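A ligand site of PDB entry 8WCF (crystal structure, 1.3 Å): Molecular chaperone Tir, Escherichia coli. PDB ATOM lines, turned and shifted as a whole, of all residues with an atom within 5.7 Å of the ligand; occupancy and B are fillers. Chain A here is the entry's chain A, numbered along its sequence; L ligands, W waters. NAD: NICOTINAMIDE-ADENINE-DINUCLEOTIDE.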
ATOM      1  N   PHE A  11       2.494   3.007  -7.303  1.00  0.00           N
ATOM      2  CA  PHE A  11       3.560   2.033  -7.104  1.00  0.00           C
ATOM      3  C   PHE A  11       4.836   2.844  -6.910  1.00  0.00           C
ATOM      4  O   PHE A  11       5.216   3.611  -7.806  1.00  0.00           O
ATOM      5  CB  PHE A  11       3.655   1.163  -8.367  1.00  0.00           C
ATOM      6  CG  PHE A  11       4.670   0.050  -8.301  1.00  0.00           C
ATOM      7  CD1 PHE A  11       6.025   0.319  -8.319  1.00  0.00           C
ATOM      8  CD2 PHE A  11       4.270  -1.277  -8.306  1.00  0.00           C
ATOM      9  CE1 PHE A  11       6.942  -0.696  -8.291  1.00  0.00           C
ATOM     10  CE2 PHE A  11       5.187  -2.292  -8.278  1.00  0.00           C
ATOM     11  CZ  PHE A  11       6.523  -2.002  -8.271  1.00  0.00           C
ATOM     12  N   TYR A  12       5.487   2.692  -5.756  1.00  0.00           N
ATOM     13  CA  TYR A  12       6.771   3.338  -5.514  1.00  0.00           C
ATOM     14  C   TYR A  12       7.889   2.437  -6.012  1.00  0.00           C
ATOM     15  O   TYR A  12       7.965   1.257  -5.620  1.00  0.00           O
ATOM     16  CB  TYR A  12       6.994   3.607  -4.026  1.00  0.00           C
ATOM     17  CG  TYR A  12       6.073   4.599  -3.378  1.00  0.00           C
ATOM     18  CD1 TYR A  12       5.905   5.882  -3.890  1.00  0.00           C
ATOM     19  CD2 TYR A  12       5.393   4.269  -2.206  1.00  0.00           C
ATOM     20  CE1 TYR A  12       5.078   6.801  -3.264  1.00  0.00           C
ATOM     21  CE2 TYR A  12       4.566   5.188  -1.580  1.00  0.00           C
ATOM     22  CZ  TYR A  12       4.405   6.443  -2.110  1.00  0.00           C
ATOM     23  OH  TYR A  12       3.584   7.357  -1.496  1.00  0.00           O
ATOM     24  N   SER A  13       8.787   2.982  -6.828  1.00  0.00           N
ATOM     25  CA  SER A  13       9.928   2.258  -7.390  1.00  0.00           C
ATOM     26  C   SER A  13      11.182   2.926  -6.851  1.00  0.00           C
ATOM     27  O   SER A  13      11.367   4.135  -7.026  1.00  0.00           O
ATOM     28  CB  SER A  13       9.857   2.336  -8.917  1.00  0.00           C
ATOM     29  OG  SER A  13      10.953   1.720  -9.531  1.00  0.00           O
ATOM     30  N   PHE A  14      12.035   2.153  -6.175  1.00  0.00           N
ATOM     31  CA  PHE A  14      13.198   2.749  -5.535  1.00  0.00           C
ATOM     32  C   PHE A  14      14.178   1.678  -5.109  1.00  0.00           C
ATOM     33  O   PHE A  14      13.873   0.490  -5.099  1.00  0.00           O
ATOM     34  CB  PHE A  14      12.794   3.631  -4.345  1.00  0.00           C
ATOM     35  CG  PHE A  14      12.095   2.886  -3.229  1.00  0.00           C
ATOM     36  CD1 PHE A  14      10.729   2.662  -3.274  1.00  0.00           C
ATOM     37  CD2 PHE A  14      12.796   2.472  -2.110  1.00  0.00           C
ATOM     38  CE1 PHE A  14      10.088   1.999  -2.237  1.00  0.00           C
ATOM     39  CE2 PHE A  14      12.156   1.819  -1.076  1.00  0.00           C
ATOM     40  CZ  PHE A  14      10.805   1.588  -1.137  1.00  0.00           C
ATOM     41  N   HIS A  15      15.379   2.139  -4.752  1.00  0.00           N
ATOM     42  CA  HIS A  15      16.466   1.305  -4.261  1.00  0.00           C
ATOM     43  C   HIS A  15      16.332   1.170  -2.745  1.00  0.00           C
ATOM     44  O   HIS A  15      16.535   2.142  -2.001  1.00  0.00           O
ATOM     45  CB  HIS A  15      17.776   1.988  -4.640  1.00  0.00           C
ATOM     46  CG  HIS A  15      18.991   1.271  -4.155  1.00  0.00           C
ATOM     47  ND1 HIS A  15      20.183   1.924  -3.898  1.00  0.00           N
ATOM     48  CD2 HIS A  15      19.200  -0.038  -3.877  1.00  0.00           C
ATOM     49  CE1 HIS A  15      21.069   1.045  -3.478  1.00  0.00           C
ATOM     50  NE2 HIS A  15      20.509  -0.158  -3.467  1.00  0.00           N
ATOM     51  N   PHE A  16      16.005  -0.022  -2.279  1.00  0.00           N
ATOM     52  CA  PHE A  16      15.626  -0.187  -0.875  1.00  0.00           C
ATOM     53  C   PHE A  16      16.790   0.080   0.069  1.00  0.00           C
ATOM     54  O   PHE A  16      16.638   0.820   1.054  1.00  0.00           O
ATOM     55  CB  PHE A  16      15.056  -1.589  -0.655  1.00  0.00           C
ATOM     56  CG  PHE A  16      13.573  -1.634  -0.761  1.00  0.00           C
ATOM     57  CD1 PHE A  16      12.948  -1.430  -1.972  1.00  0.00           C
ATOM     58  CD2 PHE A  16      12.783  -1.856   0.365  1.00  0.00           C
ATOM     59  CE1 PHE A  16      11.581  -1.450  -2.077  1.00  0.00           C
ATOM     60  CE2 PHE A  16      11.416  -1.876   0.259  1.00  0.00           C
ATOM     61  CZ  PHE A  16      10.811  -1.667  -0.961  1.00  0.00           C
ATOM     62  N   ASP A  17      17.945  -0.535  -0.170  1.00  0.00           N
ATOM     63  CA  ASP A  17      18.984  -0.497   0.862  1.00  0.00           C
ATOM     64  C   ASP A  17      19.534   0.904   1.074  1.00  0.00           C
ATOM     65  O   ASP A  17      20.036   1.190   2.172  1.00  0.00           O
ATOM     66  CB  ASP A  17      20.094  -1.502   0.537  1.00  0.00           C
ATOM     67  CG  ASP A  17      19.696  -2.929   0.857  1.00  0.00           C
ATOM     68  OD1 ASP A  17      18.679  -3.119   1.570  1.00  0.00           O
ATOM     69  OD2 ASP A  17      20.384  -3.868   0.407  1.00  0.00           O
ATOM     70  N   VAL A  20      14.999   3.309   1.516  1.00  0.00           N
ATOM     71  CA  VAL A  20      13.711   2.898   2.064  1.00  0.00           C
ATOM     72  C   VAL A  20      13.224   3.855   3.149  1.00  0.00           C
ATOM     73  O   VAL A  20      12.028   4.161   3.224  1.00  0.00           O
ATOM     74  CB  VAL A  20      13.777   1.439   2.540  1.00  0.00           C
ATOM     75  CG1 VAL A  20      14.752   1.287   3.712  1.00  0.00           C
ATOM     76  CG2 VAL A  20      12.393   0.936   2.917  1.00  0.00           C
ATOM     77  N   GLU A  36       2.430  -0.549   0.484  1.00  0.00           N
ATOM     78  CA  GLU A  36       3.529  -0.781   1.422  1.00  0.00           C
ATOM     79  C   GLU A  36       4.401  -1.929   0.933  1.00  0.00           C
ATOM     80  O   GLU A  36       3.951  -2.800   0.192  1.00  0.00           O
ATOM     81  CB  GLU A  36       2.970  -1.131   2.793  1.00  0.00           C
ATOM     82  CG  GLU A  36       2.227   0.011   3.462  1.00  0.00           C
ATOM     83  CD  GLU A  36       3.148   1.113   3.947  1.00  0.00           C
ATOM     84  OE1 GLU A  36       4.339   0.818   4.215  1.00  0.00           O
ATOM     85  OE2 GLU A  36       2.688   2.262   4.060  1.00  0.00           O
ATOM     86  N   PRO A  37       5.676  -1.961   1.336  1.00  0.00           N
ATOM     87  CA  PRO A  37       6.525  -3.083   0.918  1.00  0.00           C
ATOM     88  C   PRO A  37       6.083  -4.381   1.569  1.00  0.00           C
ATOM     89  O   PRO A  37       5.457  -4.384   2.627  1.00  0.00           O
ATOM     90  CB  PRO A  37       7.921  -2.684   1.407  1.00  0.00           C
ATOM     91  CG  PRO A  37       7.841  -1.228   1.807  1.00  0.00           C
ATOM     92  CD  PRO A  37       6.395  -0.985   2.172  1.00  0.00           C
ATOM     93  N   VAL A  38       6.414  -5.497   0.924  1.00  0.00           N
ATOM     94  CA  VAL A  38       6.284  -6.794   1.588  1.00  0.00           C
ATOM     95  C   VAL A  38       7.414  -6.924   2.600  1.00  0.00           C
ATOM     96  O   VAL A  38       8.359  -6.129   2.615  1.00  0.00           O
ATOM     97  CB  VAL A  38       6.275  -7.969   0.589  1.00  0.00           C
ATOM     98  CG1 VAL A  38       5.075  -7.870  -0.352  1.00  0.00           C
ATOM     99  CG2 VAL A  38       7.590  -8.040  -0.174  1.00  0.00           C
ATOM    100  N   SER A  39       7.337  -7.923   3.469  1.00  0.00           N
ATOM    101  CA  SER A  39       8.362  -8.087   4.489  1.00  0.00           C
ATOM    102  C   SER A  39       9.677  -8.552   3.856  1.00  0.00           C
ATOM    103  O   SER A  39       9.684  -9.095   2.750  1.00  0.00           O
ATOM    104  CB  SER A  39       7.921  -9.109   5.518  1.00  0.00           C
ATOM    105  OG  SER A  39       8.028 -10.409   4.991  1.00  0.00           O
ATOM    106  N   PRO A  40      10.809  -8.366   4.555  1.00  0.00           N
ATOM    107  CA  PRO A  40      12.081  -8.826   3.983  1.00  0.00           C
ATOM    108  C   PRO A  40      12.101 -10.307   3.649  1.00  0.00           C
ATOM    109  O   PRO A  40      12.614 -10.699   2.592  1.00  0.00           O
ATOM    110  CB  PRO A  40      13.102  -8.454   5.062  1.00  0.00           C
ATOM    111  CG  PRO A  40      12.482  -7.302   5.788  1.00  0.00           C
ATOM    112  CD  PRO A  40      11.003  -7.627   5.805  1.00  0.00           C
ATOM    113  N   TRP A  43      10.129 -10.838   0.506  1.00  0.00           N
ATOM    114  CA  TRP A  43      10.900 -10.425  -0.658  1.00  0.00           C
ATOM    115  C   TRP A  43      11.936 -11.485  -1.027  1.00  0.00           C
ATOM    116  O   TRP A  43      12.130 -11.786  -2.215  1.00  0.00           O
ATOM    117  CB  TRP A  43      11.556  -9.049  -0.407  1.00  0.00           C
ATOM    118  CG  TRP A  43      12.169  -8.524  -1.665  1.00  0.00           C
ATOM    119  CD1 TRP A  43      13.490  -8.287  -1.905  1.00  0.00           C
ATOM    120  CD2 TRP A  43      11.480  -8.218  -2.885  1.00  0.00           C
ATOM    121  NE1 TRP A  43      13.670  -7.858  -3.201  1.00  0.00           N
ATOM    122  CE2 TRP A  43      12.453  -7.806  -3.823  1.00  0.00           C
ATOM    123  CE3 TRP A  43      10.146  -8.258  -3.278  1.00  0.00           C
ATOM    124  CZ2 TRP A  43      12.116  -7.428  -5.120  1.00  0.00           C
ATOM    125  CZ3 TRP A  43       9.822  -7.880  -4.570  1.00  0.00           C
ATOM    126  CH2 TRP A  43      10.803  -7.481  -5.475  1.00  0.00           C
ATOM    127  N   GLU A  44      12.614 -12.062  -0.036  1.00  0.00           N
ATOM    128  CA  GLU A  44      13.602 -13.096  -0.345  1.00  0.00           C
ATOM    129  C   GLU A  44      12.945 -14.299  -1.029  1.00  0.00           C
ATOM    130  O   GLU A  44      13.509 -14.872  -1.963  1.00  0.00           O
ATOM    131  CB  GLU A  44      14.327 -13.507   0.929  1.00  0.00           C
ATOM    132  CG  GLU A  44      15.289 -12.429   1.425  1.00  0.00           C
ATOM    133  CD  GLU A  44      16.246 -11.947   0.332  1.00  0.00           C
ATOM    134  OE1 GLU A  44      16.973 -12.797  -0.224  1.00  0.00           O
ATOM    135  OE2 GLU A  44      16.264 -10.733   0.025  1.00  0.00           O
ATOM    136  N   LYS A  47      12.246 -13.350  -4.620  1.00  0.00           N
ATOM    137  CA  LYS A  47      13.474 -13.242  -5.391  1.00  0.00           C
ATOM    138  C   LYS A  47      14.077 -14.594  -5.748  1.00  0.00           C
ATOM    139  O   LYS A  47      15.103 -14.636  -6.452  1.00  0.00           O
ATOM    140  CB  LYS A  47      14.522 -12.446  -4.606  1.00  0.00           C
ATOM    141  CG  LYS A  47      14.260 -10.946  -4.530  1.00  0.00           C
ATOM    142  CD  LYS A  47      14.743 -10.211  -5.784  1.00  0.00           C
ATOM    143  CE  LYS A  47      16.255 -10.273  -5.977  1.00  0.00           C
ATOM    144  NZ  LYS A  47      17.019  -9.397  -5.035  1.00  0.00           N
ATOM    145  N   TRP A  56       5.273 -10.669  -9.137  1.00  0.00           N
ATOM    146  CA  TRP A  56       4.974  -9.757  -8.043  1.00  0.00           C
ATOM    147  C   TRP A  56       4.885  -8.322  -8.536  1.00  0.00           C
ATOM    148  O   TRP A  56       3.944  -7.587  -8.184  1.00  0.00           O
ATOM    149  CB  TRP A  56       6.021  -9.885  -6.929  1.00  0.00           C
ATOM    150  CG  TRP A  56       5.724  -8.965  -5.805  1.00  0.00           C
ATOM    151  CD1 TRP A  56       4.935  -9.220  -4.716  1.00  0.00           C
ATOM    152  CD2 TRP A  56       6.189  -7.627  -5.663  1.00  0.00           C
ATOM    153  NE1 TRP A  56       4.879  -8.115  -3.906  1.00  0.00           N
ATOM    154  CE2 TRP A  56       5.650  -7.121  -4.456  1.00  0.00           C
ATOM    155  CE3 TRP A  56       7.006  -6.790  -6.428  1.00  0.00           C
ATOM    156  CZ2 TRP A  56       5.896  -5.825  -4.011  1.00  0.00           C
ATOM    157  CZ3 TRP A  56       7.250  -5.503  -5.979  1.00  0.00           C
ATOM    158  CH2 TRP A  56       6.700  -5.030  -4.782  1.00  0.00           C
ATOM    159  N   ILE A  57       5.851  -7.893  -9.353  1.00  0.00           N
ATOM    160  CA  ILE A  57       5.821  -6.534  -9.898  1.00  0.00           C
ATOM    161  C   ILE A  57       4.567  -6.331 -10.730  1.00  0.00           C
ATOM    162  O   ILE A  57       3.833  -5.345 -10.561  1.00  0.00           O
ATOM    163  CB  ILE A  57       7.088  -6.246 -10.718  1.00  0.00           C
ATOM    164  CG1 ILE A  57       8.313  -6.185  -9.794  1.00  0.00           C
ATOM    165  CG2 ILE A  57       6.924  -4.959 -11.523  1.00  0.00           C
ATOM    166  CD1 ILE A  57       9.640  -6.096 -10.547  1.00  0.00           C
ATOM    167  N   ARG A  78      19.534   0.136 -10.812  1.00  0.00           N
ATOM    168  CA  ARG A  78      18.849  -1.032 -10.234  1.00  0.00           C
ATOM    169  C   ARG A  78      18.071  -1.769 -11.315  1.00  0.00           C
ATOM    170  O   ARG A  78      17.168  -1.182 -11.934  1.00  0.00           O
ATOM    171  CB  ARG A  78      17.919  -0.619  -9.105  1.00  0.00           C
ATOM    172  CG  ARG A  78      18.600   0.172  -7.996  1.00  0.00           C
ATOM    173  CD  ARG A  78      19.840  -0.512  -7.463  1.00  0.00           C
ATOM    174  NE  ARG A  78      19.528  -1.769  -6.787  1.00  0.00           N
ATOM    175  CZ  ARG A  78      20.431  -2.565  -6.228  1.00  0.00           C
ATOM    176  NH1 ARG A  78      21.706  -2.229  -6.273  1.00  0.00           N
ATOM    177  NH2 ARG A  78      20.053  -3.676  -5.627  1.00  0.00           N
ATOM    178  N   PRO A  79      18.367  -3.054 -11.570  1.00  0.00           N
ATOM    179  CA  PRO A  79      17.697  -3.728 -12.701  1.00  0.00           C
ATOM    180  C   PRO A  79      16.192  -3.854 -12.566  1.00  0.00           C
ATOM    181  O   PRO A  79      15.478  -3.765 -13.577  1.00  0.00           O
ATOM    182  CB  PRO A  79      18.399  -5.091 -12.775  1.00  0.00           C
ATOM    183  CG  PRO A  79      19.044  -5.269 -11.434  1.00  0.00           C
ATOM    184  CD  PRO A  79      19.390  -3.892 -10.951  1.00  0.00           C
ATOM    185  N   TRP A  80      15.660  -4.036 -11.359  1.00  0.00           N
ATOM    186  CA  TRP A  80      14.207  -4.153 -11.237  1.00  0.00           C
ATOM    187  C   TRP A  80      13.514  -2.804 -11.309  1.00  0.00           C
ATOM    188  O   TRP A  80      12.348  -2.734 -11.711  1.00  0.00           O
ATOM    189  CB  TRP A  80      13.845  -4.936  -9.977  1.00  0.00           C
ATOM    190  CG  TRP A  80      14.216  -6.389 -10.089  1.00  0.00           C
ATOM    191  CD1 TRP A  80      15.136  -7.070  -9.354  1.00  0.00           C
ATOM    192  CD2 TRP A  80      13.669  -7.335 -11.016  1.00  0.00           C
ATOM    193  NE1 TRP A  80      15.188  -8.376  -9.756  1.00  0.00           N
ATOM    194  CE2 TRP A  80      14.298  -8.571 -10.778  1.00  0.00           C
ATOM    195  CE3 TRP A  80      12.709  -7.263 -12.030  1.00  0.00           C
ATOM    196  CZ2 TRP A  80      13.992  -9.711 -11.504  1.00  0.00           C
ATOM    197  CZ3 TRP A  80      12.407  -8.402 -12.746  1.00  0.00           C
ATOM    198  CH2 TRP A  80      13.034  -9.614 -12.469  1.00  0.00           C
ATOM    199  N   VAL A  81      14.198  -1.717 -10.953  1.00  0.00           N
ATOM    200  CA  VAL A  81      13.652  -0.392 -11.237  1.00  0.00           C
ATOM    201  C   VAL A  81      13.472  -0.217 -12.741  1.00  0.00           C
ATOM    202  O   VAL A  81      12.443   0.265 -13.214  1.00  0.00           O
ATOM    203  CB  VAL A  81      14.523   0.716 -10.621  1.00  0.00           C
ATOM    204  CG1 VAL A  81      14.056   2.091 -11.118  1.00  0.00           C
ATOM    205  CG2 VAL A  81      14.483   0.651  -9.107  1.00  0.00           C
ATOM    206  N   GLU A  84      10.437  -2.151 -13.817  1.00  0.00           N
ATOM    207  CA  GLU A  84       9.207  -1.508 -13.353  1.00  0.00           C
ATOM    208  C   GLU A  84       8.855  -0.292 -14.204  1.00  0.00           C
ATOM    209  O   GLU A  84       7.694  -0.109 -14.581  1.00  0.00           O
ATOM    210  CB  GLU A  84       9.365  -1.121 -11.889  1.00  0.00           C
ATOM    211  CG  GLU A  84       9.315  -2.340 -10.999  1.00  0.00           C
ATOM    212  CD  GLU A  84       9.881  -2.131  -9.609  1.00  0.00           C
ATOM    213  OE1 GLU A  84      10.377  -1.031  -9.299  1.00  0.00           O
ATOM    214  OE2 GLU A  84       9.802  -3.103  -8.824  1.00  0.00           O
HETATM  215  PA  NAD L   1      16.654  -5.683  -4.413  1.00  0.00           P
HETATM  216  O1A NAD L   1      18.027  -5.497  -4.897  1.00  0.00           O
HETATM  217  O2A NAD L   1      15.922  -7.000  -4.614  1.00  0.00           O
HETATM  218  O5B NAD L   1      16.560  -5.319  -2.871  1.00  0.00           O
HETATM  219  C5B NAD L   1      17.051  -6.320  -1.941  1.00  0.00           C
HETATM  220  C4B NAD L   1      17.114  -5.646  -0.585  1.00  0.00           C
HETATM  221  O4B NAD L   1      15.847  -5.223  -0.063  1.00  0.00           O
HETATM  222  C3B NAD L   1      17.720  -6.519   0.542  1.00  0.00           C
HETATM  223  O3B NAD L   1      19.103  -6.219   0.671  1.00  0.00           O
HETATM  224  C2B NAD L   1      16.922  -6.210   1.807  1.00  0.00           C
HETATM  225  O2B NAD L   1      17.669  -5.507   2.798  1.00  0.00           O
HETATM  226  C1B NAD L   1      15.899  -5.174   1.351  1.00  0.00           C
HETATM  227  N9A NAD L   1      14.514  -5.291   1.812  1.00  0.00           N
HETATM  228  C8A NAD L   1      13.595  -6.218   1.450  1.00  0.00           C
HETATM  229  N7A NAD L   1      12.439  -5.988   2.052  1.00  0.00           N
HETATM  230  C5A NAD L   1      12.584  -4.851   2.790  1.00  0.00           C
HETATM  231  C6A NAD L   1      11.716  -4.060   3.666  1.00  0.00           C
HETATM  232  N6A NAD L   1      10.440  -4.469   3.852  1.00  0.00           N
HETATM  233  N1A NAD L   1      12.236  -2.945   4.274  1.00  0.00           N
HETATM  234  C2A NAD L   1      13.507  -2.581   4.079  1.00  0.00           C
HETATM  235  N3A NAD L   1      14.334  -3.266   3.284  1.00  0.00           N
HETATM  236  C4A NAD L   1      13.925  -4.400   2.634  1.00  0.00           C
HETATM  237  O3  NAD L   1      15.730  -4.535  -5.039  1.00  0.00           O
HETATM  238  PN  NAD L   1      15.992  -2.922  -5.202  1.00  0.00           P
HETATM  239  O1N NAD L   1      16.849  -2.688  -6.393  1.00  0.00           O
HETATM  240  O2N NAD L   1      16.356  -2.304  -3.849  1.00  0.00           O
HETATM  241  O5D NAD L   1      14.508  -2.495  -5.558  1.00  0.00           O
HETATM  242  C5D NAD L   1      14.003  -2.615  -6.873  1.00  0.00           C
HETATM  243  C4D NAD L   1      12.511  -2.839  -6.842  1.00  0.00           C
HETATM  244  O4D NAD L   1      12.151  -4.163  -6.341  1.00  0.00           O
HETATM  245  C3D NAD L   1      11.724  -1.860  -5.969  1.00  0.00           C
HETATM  246  O3D NAD L   1      11.346  -0.681  -6.712  1.00  0.00           O
HETATM  247  C2D NAD L   1      10.531  -2.705  -5.511  1.00  0.00           C
HETATM  248  O2D NAD L   1       9.453  -2.629  -6.431  1.00  0.00           O
HETATM  249  C1D NAD L   1      11.073  -4.119  -5.448  1.00  0.00           C
HETATM  250  N1N NAD L   1      11.490  -4.430  -4.067  1.00  0.00           N
HETATM  251  C2N NAD L   1      10.485  -4.607  -3.207  1.00  0.00           C
HETATM  252  C3N NAD L   1      10.777  -4.830  -1.872  1.00  0.00           C
HETATM  253  C7N NAD L   1       9.666  -5.072  -0.896  1.00  0.00           C
HETATM  254  O7N NAD L   1       8.515  -4.758  -1.186  1.00  0.00           O
HETATM  255  N7N NAD L   1       9.965  -5.632   0.307  1.00  0.00           N
HETATM  256  C4N NAD L   1      12.098  -4.950  -1.490  1.00  0.00           C
HETATM  257  C5N NAD L   1      13.111  -4.716  -2.401  1.00  0.00           C
HETATM  258  C6N NAD L   1      12.780  -4.476  -3.734  1.00  0.00           C
HETATM  259  O   HOH W   1       7.510  -1.383  -5.010  1.00  0.00           O
HETATM  260  O   HOH W   2      18.449  -6.213  -7.763  1.00  0.00           O
HETATM  261  O   HOH W   3       7.690  -2.236  -2.348  1.00  0.00           O
HETATM  262  O   HOH W   4      14.834  -9.241   1.569  1.00  0.00           O
HETATM  263  O   HOH W   5      16.958  -4.132  -8.723  1.00  0.00           O
HETATM  264  O   HOH W   6      18.377  -2.653  -2.059  1.00  0.00           O
HETATM  265  O   HOH W   7      15.687  -5.810   5.107  1.00  0.00           O
HETATM  266  O   HOH W   8      10.604  -1.061   5.583  1.00  0.00           O
HETATM  267  O   HOH W   9      20.264  -4.573  -2.544  1.00  0.00           O
HETATM  268  O   HOH W  10      16.989  -2.118   3.689  1.00  0.00           O
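The side-chain amino group (NZ) of Lys 47 is in salt-bridge range of an oxygen (O2A) of the ligand (2.7 Å).
An oxygen (O2A) of the ligand is in hydrogen-bond range of the indole nitrogen of Trp 43 (2.8 Å).
The backbone NH of Phe 14 is in hydrogen-bond range of an oxygen (O3D) of the ligand (3.0 Å).
The backbone NH (N) of Phe 16 sits at hydrogen-bond distance from an oxygen (O2N) of the ligand, at 2.8 Å.
O3D of the ligand sits at hydrogen-bond distance from O of Phe 14 (3.2 Å).
The backbone carbonyl oxygen of Val 38 lies within hydrogen-bond range of a nitrogen (N7N) of the ligand, 2.9 Å away.
An oxygen (O3B) of the ligand is in hydrogen-bond range of the side-chain carboxylate (OD2) of Asp 17.
The side-chain carboxylate of Glu 84 is in hydrogen-bond range of an oxygen (O2D) of the ligand.
The guanidinium group of Arg 78 is in salt-bridge range of an oxygen (O1A) of the ligand (2.8 Å).
The backbone NH (N) of Val 38 is in hydrogen-bond range of an oxygen (O7N) of the ligand (3.1 Å).
OE1 of Glu 84 is in hydrogen-bond range of OG of Ser 13.
Phe 11 touches the ligand.
Ser 13 touches the ligand (CA to O3D, 3.3 Å).
His 15 touches the ligand (CA to O2N, 3.6 Å).
Val 20 touches the ligand (CG2 to C2A, 3.9 Å).
Pro 37 touches the ligand.
Pro 40 touches the ligand.
Trp 56 touches the ligand.
Trp 80 touches the ligand (CB to C5D, 3.9 Å).
Val 81 touches the ligand.
Hydrophobic or aromatic side chains that line the ligand: Phe 11, His 15, Phe 16, Val 20, Pro 37, Val 38, Pro 40, Trp 43, Trp 56, Trp 80 and Val 81.
17 residues have an atom within 4 Å of the ligand: Phe 11, Ser 13, Phe 14, His 15, Phe 16, Asp 17, Val 20, Pro 37, Val 38, Pro 40, Trp 43, Lys 47, Trp 56, Arg 78, Trp 80, Val 81 and Glu 84.
Water W1 bridges O2D of the ligand (2.7 Å) and O of Tyr 12 (2.7 Å).
Water W6 bridges an oxygen (O2N) of the ligand (2.7 Å) and the backbone NH of Asp 17 (2.9 Å).
Water W5 bridges an oxygen (O1N) of the ligand (2.7 Å) and the backbone NH of Trp 80 (2.9 Å).
Water W10 lies within hydrogen-bond range of OD1 of Asp 17 and N3A of the ligand.
Water W4 bridges the side-chain carboxylate (OE2) of Glu 44 (2.6 Å) and the backbone carbonyl oxygen (O) of Pro 40 (2.8 Å).
Water W9 lies within hydrogen-bond range of the side-chain carboxylate of Asp 17, the guanidinium group of Arg 78 and an oxygen (O1A) of the ligand.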
